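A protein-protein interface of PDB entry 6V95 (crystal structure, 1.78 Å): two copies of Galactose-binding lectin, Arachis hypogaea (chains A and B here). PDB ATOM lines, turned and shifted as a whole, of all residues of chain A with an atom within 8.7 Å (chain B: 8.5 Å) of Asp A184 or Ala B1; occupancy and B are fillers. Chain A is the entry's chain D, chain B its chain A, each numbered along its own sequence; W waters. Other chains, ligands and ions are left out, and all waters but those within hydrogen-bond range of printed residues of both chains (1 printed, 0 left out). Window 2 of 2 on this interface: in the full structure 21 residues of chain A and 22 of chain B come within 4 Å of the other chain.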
ATOM      1  N   TRP A 153      -6.824  13.737   9.928  1.00  0.00           N
ATOM      2  CA  TRP A 153      -5.761  12.880  10.417  1.00  0.00           C
ATOM      3  C   TRP A 153      -4.474  13.726  10.363  1.00  0.00           C
ATOM      4  O   TRP A 153      -4.545  14.932  10.061  1.00  0.00           O
ATOM      5  CB  TRP A 153      -5.735  11.596   9.538  1.00  0.00           C
ATOM      6  CG  TRP A 153      -4.618  10.636   9.796  1.00  0.00           C
ATOM      7  CD1 TRP A 153      -4.398   9.904  10.924  1.00  0.00           C
ATOM      8  CD2 TRP A 153      -3.588  10.270   8.873  1.00  0.00           C
ATOM      9  NE1 TRP A 153      -3.269   9.132  10.771  1.00  0.00           N
ATOM     10  CE2 TRP A 153      -2.740   9.353   9.531  1.00  0.00           C
ATOM     11  CE3 TRP A 153      -3.287  10.647   7.558  1.00  0.00           C
ATOM     12  CZ2 TRP A 153      -1.633   8.761   8.899  1.00  0.00           C
ATOM     13  CZ3 TRP A 153      -2.157  10.101   6.947  1.00  0.00           C
ATOM     14  CH2 TRP A 153      -1.351   9.165   7.613  1.00  0.00           C
ATOM     15  N   VAL A 161       2.945   3.799  11.199  1.00  0.00           N
ATOM     16  CA  VAL A 161       1.468   3.849  11.328  1.00  0.00           C
ATOM     17  C   VAL A 161       0.912   2.420  11.138  1.00  0.00           C
ATOM     18  O   VAL A 161       1.310   1.733  10.213  1.00  0.00           O
ATOM     19  CB  VAL A 161       0.836   4.849  10.306  1.00  0.00           C
ATOM     20  CG1 VAL A 161      -0.694   4.869  10.419  1.00  0.00           C
ATOM     21  CG2 VAL A 161       1.394   6.263  10.476  1.00  0.00           C
ATOM     22  N   LYS A 162      -0.005   1.991  12.012  1.00  0.00           N
ATOM     23  CA  LYS A 162      -0.691   0.696  11.943  1.00  0.00           C
ATOM     24  C   LYS A 162      -2.147   0.920  11.534  1.00  0.00           C
ATOM     25  O   LYS A 162      -2.805   1.845  12.014  1.00  0.00           O
ATOM     26  CB  LYS A 162      -0.628  -0.058  13.294  1.00  0.00           C
ATOM     27  CG  LYS A 162       0.775  -0.378  13.796  1.00  0.00           C
ATOM     28  CD  LYS A 162       0.741  -1.483  14.840  1.00  0.00           C
ATOM     29  CE  LYS A 162       0.620  -1.017  16.274  1.00  0.00           C
ATOM     30  NZ  LYS A 162       0.453  -2.165  17.204  1.00  0.00           N
ATOM     31  N   ALA A 177      -9.488   1.510  11.241  1.00  0.00           N
ATOM     32  CA  ALA A 177      -8.889   2.020  12.490  1.00  0.00           C
ATOM     33  C   ALA A 177      -7.402   2.245  12.239  1.00  0.00           C
ATOM     34  O   ALA A 177      -6.684   1.319  11.790  1.00  0.00           O
ATOM     35  CB  ALA A 177      -9.123   1.068  13.661  1.00  0.00           C
ATOM     36  N   VAL A 178      -6.952   3.501  12.436  1.00  0.00           N
ATOM     37  CA  VAL A 178      -5.574   3.949  12.200  1.00  0.00           C
ATOM     38  C   VAL A 178      -4.935   4.292  13.538  1.00  0.00           C
ATOM     39  O   VAL A 178      -5.478   5.138  14.257  1.00  0.00           O
ATOM     40  CB  VAL A 178      -5.556   5.161  11.231  1.00  0.00           C
ATOM     41  CG1 VAL A 178      -4.123   5.532  10.849  1.00  0.00           C
ATOM     42  CG2 VAL A 178      -6.379   4.884   9.976  1.00  0.00           C
ATOM     43  N   THR A 179      -3.829   3.615  13.892  1.00  0.00           N
ATOM     44  CA  THR A 179      -3.114   3.823  15.161  1.00  0.00           C
ATOM     45  C   THR A 179      -1.893   4.646  14.886  1.00  0.00           C
ATOM     46  O   THR A 179      -0.949   4.157  14.250  1.00  0.00           O
ATOM     47  CB  THR A 179      -2.763   2.489  15.881  1.00  0.00           C
ATOM     48  OG1 THR A 179      -3.955   1.729  16.066  1.00  0.00           O
ATOM     49  CG2 THR A 179      -2.133   2.724  17.266  1.00  0.00           C
ATOM     50  N   ASN A 180      -1.923   5.891  15.381  1.00  0.00           N
ATOM     51  CA  ASN A 180      -0.881   6.903  15.273  1.00  0.00           C
ATOM     52  C   ASN A 180       0.268   6.664  16.276  1.00  0.00           C
ATOM     53  O   ASN A 180       0.174   5.804  17.166  1.00  0.00           O
ATOM     54  CB  ASN A 180      -1.486   8.299  15.474  1.00  0.00           C
ATOM     55  CG  ASN A 180      -2.475   8.646  14.403  1.00  0.00           C
ATOM     56  OD1 ASN A 180      -2.131   8.667  13.220  1.00  0.00           O
ATOM     57  ND2 ASN A 180      -3.752   8.831  14.786  1.00  0.00           N
ATOM     58  N   ASP A 181       1.363   7.417  16.085  1.00  0.00           N
ATOM     59  CA  ASP A 181       2.568   7.368  16.913  1.00  0.00           C
ATOM     60  C   ASP A 181       2.285   7.933  18.311  1.00  0.00           C
ATOM     61  O   ASP A 181       2.732   7.339  19.294  1.00  0.00           O
ATOM     62  CB  ASP A 181       3.710   8.132  16.215  1.00  0.00           C
ATOM     63  CG  ASP A 181       5.013   8.230  16.984  1.00  0.00           C
ATOM     64  OD1 ASP A 181       5.669   7.180  17.176  1.00  0.00           O
ATOM     65  OD2 ASP A 181       5.414   9.368  17.333  1.00  0.00           O
ATOM     66  N   ASN A 182       1.479   9.022  18.409  1.00  0.00           N
ATOM     67  CA  ASN A 182       1.109   9.665  19.683  1.00  0.00           C
ATOM     68  C   ASN A 182       0.094   8.821  20.516  1.00  0.00           C
ATOM     69  O   ASN A 182      -0.338   9.265  21.588  1.00  0.00           O
ATOM     70  CB  ASN A 182       0.588  11.096  19.439  1.00  0.00           C
ATOM     71  CG  ASN A 182      -0.893  11.296  19.168  1.00  0.00           C
ATOM     72  OD1 ASN A 182      -1.574  10.551  18.446  1.00  0.00           O
ATOM     73  ND2 ASN A 182      -1.392  12.399  19.676  1.00  0.00           N
ATOM     74  N   GLY A 183      -0.251   7.627  20.012  1.00  0.00           N
ATOM     75  CA  GLY A 183      -1.128   6.667  20.674  1.00  0.00           C
ATOM     76  C   GLY A 183      -2.599   6.722  20.324  1.00  0.00           C
ATOM     77  O   GLY A 183      -3.295   5.727  20.525  1.00  0.00           O
ATOM     78  N   ASP A 184      -3.079   7.864  19.808  1.00  0.00           N
ATOM     79  CA  ASP A 184      -4.477   8.065  19.434  1.00  0.00           C
ATOM     80  C   ASP A 184      -4.875   7.159  18.267  1.00  0.00           C
ATOM     81  O   ASP A 184      -4.047   6.844  17.409  1.00  0.00           O
ATOM     82  CB  ASP A 184      -4.757   9.525  19.034  1.00  0.00           C
ATOM     83  CG  ASP A 184      -4.735  10.570  20.148  1.00  0.00           C
ATOM     84  OD1 ASP A 184      -4.232  10.259  21.244  1.00  0.00           O
ATOM     85  OD2 ASP A 184      -5.249  11.681  19.922  1.00  0.00           O
ATOM     86  N   ILE A 185      -6.137   6.769  18.256  1.00  0.00           N
ATOM     87  CA  ILE A 185      -6.744   6.025  17.165  1.00  0.00           C
ATOM     88  C   ILE A 185      -7.680   6.957  16.390  1.00  0.00           C
ATOM     89  O   ILE A 185      -8.356   7.824  16.971  1.00  0.00           O
ATOM     90  CB  ILE A 185      -7.447   4.690  17.529  1.00  0.00           C
ATOM     91  CG1 ILE A 185      -8.413   4.824  18.698  1.00  0.00           C
ATOM     92  CG2 ILE A 185      -6.444   3.575  17.728  1.00  0.00           C
ATOM     93  CD1 ILE A 185      -9.732   4.628  18.250  1.00  0.00           C
ATOM     94  N   THR A 186      -7.645   6.818  15.063  1.00  0.00           N
ATOM     95  CA  THR A 186      -8.510   7.543  14.126  1.00  0.00           C
ATOM     96  C   THR A 186      -9.358   6.471  13.434  1.00  0.00           C
ATOM     97  O   THR A 186      -8.803   5.462  13.027  1.00  0.00           O
ATOM     98  CB  THR A 186      -7.658   8.336  13.124  1.00  0.00           C
ATOM     99  OG1 THR A 186      -6.761   9.183  13.827  1.00  0.00           O
ATOM    100  CG2 THR A 186      -8.495   9.157  12.133  1.00  0.00           C
ATOM    101  N   THR A 187     -10.670   6.653  13.364  1.00  0.00           N
ATOM    102  CA  THR A 187     -11.547   5.687  12.689  1.00  0.00           C
ATOM    103  C   THR A 187     -12.359   6.388  11.633  1.00  0.00           C
ATOM    104  O   THR A 187     -12.638   7.599  11.735  1.00  0.00           O
ATOM    105  CB  THR A 187     -12.477   4.909  13.640  1.00  0.00           C
ATOM    106  OG1 THR A 187     -13.466   5.774  14.196  1.00  0.00           O
ATOM    107  CG2 THR A 187     -11.744   4.123  14.712  1.00  0.00           C
ATOM    108  N   ALA B   1      -6.707  15.278  22.093  1.00  0.00           N
ATOM    109  CA  ALA B   1      -7.675  14.203  22.299  1.00  0.00           C
ATOM    110  C   ALA B   1      -7.337  13.353  23.539  1.00  0.00           C
ATOM    111  O   ALA B   1      -6.208  13.360  24.021  1.00  0.00           O
ATOM    112  CB  ALA B   1      -7.761  13.327  21.061  1.00  0.00           C
ATOM    113  N   GLU B   2      -8.348  12.679  24.079  1.00  0.00           N
ATOM    114  CA  GLU B   2      -8.238  11.866  25.294  1.00  0.00           C
ATOM    115  C   GLU B   2      -8.191  10.401  24.873  1.00  0.00           C
ATOM    116  O   GLU B   2      -9.171   9.885  24.322  1.00  0.00           O
ATOM    117  CB  GLU B   2      -9.445  12.166  26.209  1.00  0.00           C
ATOM    118  CG  GLU B   2      -9.502  11.421  27.526  1.00  0.00           C
ATOM    119  CD  GLU B   2     -10.683  11.863  28.362  1.00  0.00           C
ATOM    120  OE1 GLU B   2     -10.691  13.039  28.775  1.00  0.00           O
ATOM    121  OE2 GLU B   2     -11.627  11.069  28.557  1.00  0.00           O
ATOM    122  N   THR B   3      -7.075   9.738  25.177  1.00  0.00           N
ATOM    123  CA  THR B   3      -6.857   8.343  24.803  1.00  0.00           C
ATOM    124  C   THR B   3      -6.568   7.453  26.012  1.00  0.00           C
ATOM    125  O   THR B   3      -5.830   7.846  26.911  1.00  0.00           O
ATOM    126  CB  THR B   3      -5.715   8.273  23.754  1.00  0.00           C
ATOM    127  OG1 THR B   3      -6.210   8.879  22.555  1.00  0.00           O
ATOM    128  CG2 THR B   3      -5.245   6.831  23.453  1.00  0.00           C
ATOM    129  N   VAL B   4      -7.218   6.278  26.035  1.00  0.00           N
ATOM    130  CA  VAL B   4      -7.007   5.187  26.991  1.00  0.00           C
ATOM    131  C   VAL B   4      -6.393   4.041  26.186  1.00  0.00           C
ATOM    132  O   VAL B   4      -6.995   3.600  25.204  1.00  0.00           O
ATOM    133  CB  VAL B   4      -8.292   4.729  27.747  1.00  0.00           C
ATOM    134  CG1 VAL B   4      -8.014   3.478  28.596  1.00  0.00           C
ATOM    135  CG2 VAL B   4      -8.865   5.839  28.609  1.00  0.00           C
ATOM    136  N   SER B   5      -5.211   3.576  26.594  1.00  0.00           N
ATOM    137  CA  SER B   5      -4.537   2.490  25.889  1.00  0.00           C
ATOM    138  C   SER B   5      -3.916   1.502  26.860  1.00  0.00           C
ATOM    139  O   SER B   5      -3.248   1.908  27.815  1.00  0.00           O
ATOM    140  CB  SER B   5      -3.467   3.059  24.964  1.00  0.00           C
ATOM    141  OG  SER B   5      -3.099   2.106  23.988  1.00  0.00           O
ATOM    142  N   ARG B  53     -14.208   7.060  29.861  1.00  0.00           N
ATOM    143  CA  ARG B  53     -15.190   8.070  29.452  1.00  0.00           C
ATOM    144  C   ARG B  53     -15.421   7.855  27.950  1.00  0.00           C
ATOM    145  O   ARG B  53     -14.548   8.199  27.144  1.00  0.00           O
ATOM    146  CB  ARG B  53     -14.663   9.474  29.812  1.00  0.00           C
ATOM    147  CG  ARG B  53     -15.607  10.649  29.599  1.00  0.00           C
ATOM    148  CD  ARG B  53     -14.738  11.886  29.777  1.00  0.00           C
ATOM    149  NE  ARG B  53     -15.353  13.102  29.270  1.00  0.00           N
ATOM    150  CZ  ARG B  53     -14.668  14.174  28.888  1.00  0.00           C
ATOM    151  NH1 ARG B  53     -13.340  14.168  28.915  1.00  0.00           N
ATOM    152  NH2 ARG B  53     -15.304  15.254  28.459  1.00  0.00           N
ATOM    153  N   SER B  64     -14.117   6.704  19.686  1.00  0.00           N
ATOM    154  CA  SER B  64     -13.950   5.544  18.813  1.00  0.00           C
ATOM    155  C   SER B  64     -13.041   4.619  19.562  1.00  0.00           C
ATOM    156  O   SER B  64     -12.295   5.099  20.434  1.00  0.00           O
ATOM    157  CB  SER B  64     -13.340   5.929  17.462  1.00  0.00           C
ATOM    158  OG  SER B  64     -14.320   6.517  16.623  1.00  0.00           O
ATOM    159  N   LEU B  66     -10.592   0.681  19.222  1.00  0.00           N
ATOM    160  CA  LEU B  66     -10.034  -0.496  18.563  1.00  0.00           C
ATOM    161  C   LEU B  66      -9.612  -1.447  19.664  1.00  0.00           C
ATOM    162  O   LEU B  66      -8.836  -1.065  20.549  1.00  0.00           O
ATOM    163  CB  LEU B  66      -8.853  -0.144  17.650  1.00  0.00           C
ATOM    164  CG  LEU B  66      -7.999  -1.332  17.174  1.00  0.00           C
ATOM    165  CD1 LEU B  66      -8.815  -2.236  16.157  1.00  0.00           C
ATOM    166  CD2 LEU B  66      -6.708  -0.870  16.599  1.00  0.00           C
ATOM    167  N   THR B 226      -7.519   0.418  22.655  1.00  0.00           N
ATOM    168  CA  THR B 226      -7.237   1.831  22.484  1.00  0.00           C
ATOM    169  C   THR B 226      -8.547   2.540  22.188  1.00  0.00           C
ATOM    170  O   THR B 226      -9.234   2.170  21.250  1.00  0.00           O
ATOM    171  CB  THR B 226      -6.184   2.177  21.415  1.00  0.00           C
ATOM    172  OG1 THR B 226      -4.960   1.462  21.647  1.00  0.00           O
ATOM    173  CG2 THR B 226      -5.903   3.706  21.355  1.00  0.00           C
ATOM    174  N   SER B 227      -8.869   3.563  22.973  1.00  0.00           N
ATOM    175  CA  SER B 227     -10.028   4.432  22.736  1.00  0.00           C
ATOM    176  C   SER B 227      -9.523   5.855  22.625  1.00  0.00           C
ATOM    177  O   SER B 227      -8.566   6.218  23.316  1.00  0.00           O
ATOM    178  CB  SER B 227     -11.065   4.305  23.846  1.00  0.00           C
ATOM    179  OG  SER B 227     -10.594   4.830  25.080  1.00  0.00           O
ATOM    180  N   THR B 228     -10.117   6.646  21.742  1.00  0.00           N
ATOM    181  CA  THR B 228      -9.761   8.050  21.564  1.00  0.00           C
ATOM    182  C   THR B 228     -11.041   8.876  21.450  1.00  0.00           C
ATOM    183  O   THR B 228     -11.879   8.613  20.594  1.00  0.00           O
ATOM    184  CB  THR B 228      -8.823   8.262  20.369  1.00  0.00           C
ATOM    185  OG1 THR B 228      -7.610   7.561  20.609  1.00  0.00           O
ATOM    186  CG2 THR B 228      -8.512   9.739  20.115  1.00  0.00           C
ATOM    187  N   LEU B 229     -11.182   9.866  22.343  1.00  0.00           N
ATOM    188  CA  LEU B 229     -12.298  10.817  22.381  1.00  0.00           C
ATOM    189  C   LEU B 229     -11.766  12.203  21.997  1.00  0.00           C
ATOM    190  O   LEU B 229     -10.763  12.667  22.560  1.00  0.00           O
ATOM    191  CB  LEU B 229     -12.923  10.834  23.802  1.00  0.00           C
ATOM    192  CG  LEU B 229     -14.032  11.844  24.122  1.00  0.00           C
ATOM    193  CD1 LEU B 229     -15.350  11.482  23.407  1.00  0.00           C
ATOM    194  CD2 LEU B 229     -14.264  11.925  25.629  1.00  0.00           C
ATOM    195  N   ILE B 230     -12.377  12.822  20.990  1.00  0.00           N
ATOM    196  CA  ILE B 230     -12.005  14.178  20.592  1.00  0.00           C
ATOM    197  C   ILE B 230     -12.524  15.129  21.696  1.00  0.00           C
ATOM    198  O   ILE B 230     -13.698  15.060  22.067  1.00  0.00           O
ATOM    199  CB  ILE B 230     -12.563  14.513  19.179  1.00  0.00           C
ATOM    200  CG1 ILE B 230     -11.824  13.688  18.058  1.00  0.00           C
ATOM    201  CG2 ILE B 230     -12.602  16.047  18.889  1.00  0.00           C
ATOM    202  CD1 ILE B 230     -10.350  14.096  17.565  1.00  0.00           C
ATOM    203  N   THR B 231     -11.620  15.951  22.253  1.00  0.00           N
ATOM    204  CA  THR B 231     -11.907  16.937  23.303  1.00  0.00           C
ATOM    205  C   THR B 231     -11.866  18.305  22.626  1.00  0.00           C
ATOM    206  O   THR B 231     -10.792  18.740  22.199  1.00  0.00           O
ATOM    207  CB  THR B 231     -10.930  16.797  24.487  1.00  0.00           C
ATOM    208  OG1 THR B 231      -9.585  16.757  23.991  1.00  0.00           O
ATOM    209  CG2 THR B 231     -11.219  15.577  25.351  1.00  0.00           C
ATOM    210  N   THR B 232     -13.046  18.879  22.361  1.00  0.00           N
ATOM    211  CA  THR B 232     -13.155  20.132  21.622  1.00  0.00           C
ATOM    212  C   THR B 232     -14.138  21.069  22.333  1.00  0.00           C
ATOM    213  O   THR B 232     -13.732  21.834  23.203  1.00  0.00           O
ATOM    214  CB  THR B 232     -13.533  19.835  20.144  1.00  0.00           C
ATOM    215  OG1 THR B 232     -13.245  20.967  19.324  1.00  0.00           O
ATOM    216  CG2 THR B 232     -14.987  19.394  19.961  1.00  0.00           C
HETATM  217  O   HOH W   1      -2.625   3.220  21.277  1.00  0.00           O
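Water W1 lies within hydrogen-bond range of the backbone carbonyl oxygen (O) of Gly A183 (2.7 Å), the side-chain hydroxyl (OG1) of Thr B226 (2.9 Å) and the side-chain hydroxyl (OG) of Ser B5 (3.0 Å).
Of chain B, only Thr B3 and Thr B226 come within 4 Å of Gly A183.
Asp A184 touches just these residues of chain B: Ala B1, Thr B3 and Thr B228.
Printed residues of chain B within 4 Å of Thr A187: Ser B64.
Of chain A, only Asp A184 comes within 4 Å of Ala B1.
Printed residues of chain A within 4 Å of Thr B3: Gly A183 (3.7 Å) and Asp A184 (2.7 Å).
Of the printed residues of chain A, Leu B66 touches Thr A179.
The nearest residue of chain B that does not touch Asp A184 is Thr B226 (4.7 Å).
The nearest residue of chain A that does not touch Ala B1 is Asn A182 (6.5 Å).
No position is printed for both chains.
Of the 10 pairs that touch across the chains among the printed residues, none has its exchanged pair printed and touching as well.
N of Leu B66 is in hydrogen-bond range of O of Thr B226 (2.9 Å).
The side-chain amide nitrogen of Asn A180 sits at hydrogen-bond distance from the backbone carbonyl oxygen of Asp A184 (3.3 Å).
O of Lys A162 is in hydrogen-bond range of N of Thr A179, at 2.8 Å.
O of Ser B64 lies within hydrogen-bond range of N of Thr B228 (3.0 Å).
OG1 of Thr B3 lies within hydrogen-bond range of OG1 of Thr B228 (2.7 Å).
The side-chain amide oxygen (OD1) of Asn A182 is in hydrogen-bond range of the backbone NH (N) of Asp A184 (3.4 Å).
Among the printed residues, pairs that only touch across the chains: Asp A184 with Ala B1 (3.2 Å), Asp A184 with Thr B228 (3.4 Å), Ile A185 with Ser B64 (3.4 Å), Gly A183 with Thr B226 (3.4 Å), Ile A185 with Thr B226 (3.7 Å), Gly A183 with Thr B3 (3.7 Å) and Thr A179 with Leu B66 (3.8 Å).
The side-chain hydroxyl (OG1) of Thr B228 lies within hydrogen-bond range of the backbone NH (N) of Ile A185, at 2.9 Å.
The side-chain hydroxyl (OG1) of Thr B3 lies within hydrogen-bond range of the side-chain carboxylate (OD1) of Asp A184, at 2.7 Å.
The side-chain hydroxyl of Ser B64 lies within hydrogen-bond range of the side-chain hydroxyl of Thr A187 (2.7 Å).
Printed residues of chain A that touch a printed residue of chain B: Thr A179, Gly A183, Asp A184, Ile A185 and Thr A187.
Of the 15 printed residues of chain B, 6 touch a printed residue of chain A.
Among the printed residues, 10 pairs touch across the chains.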
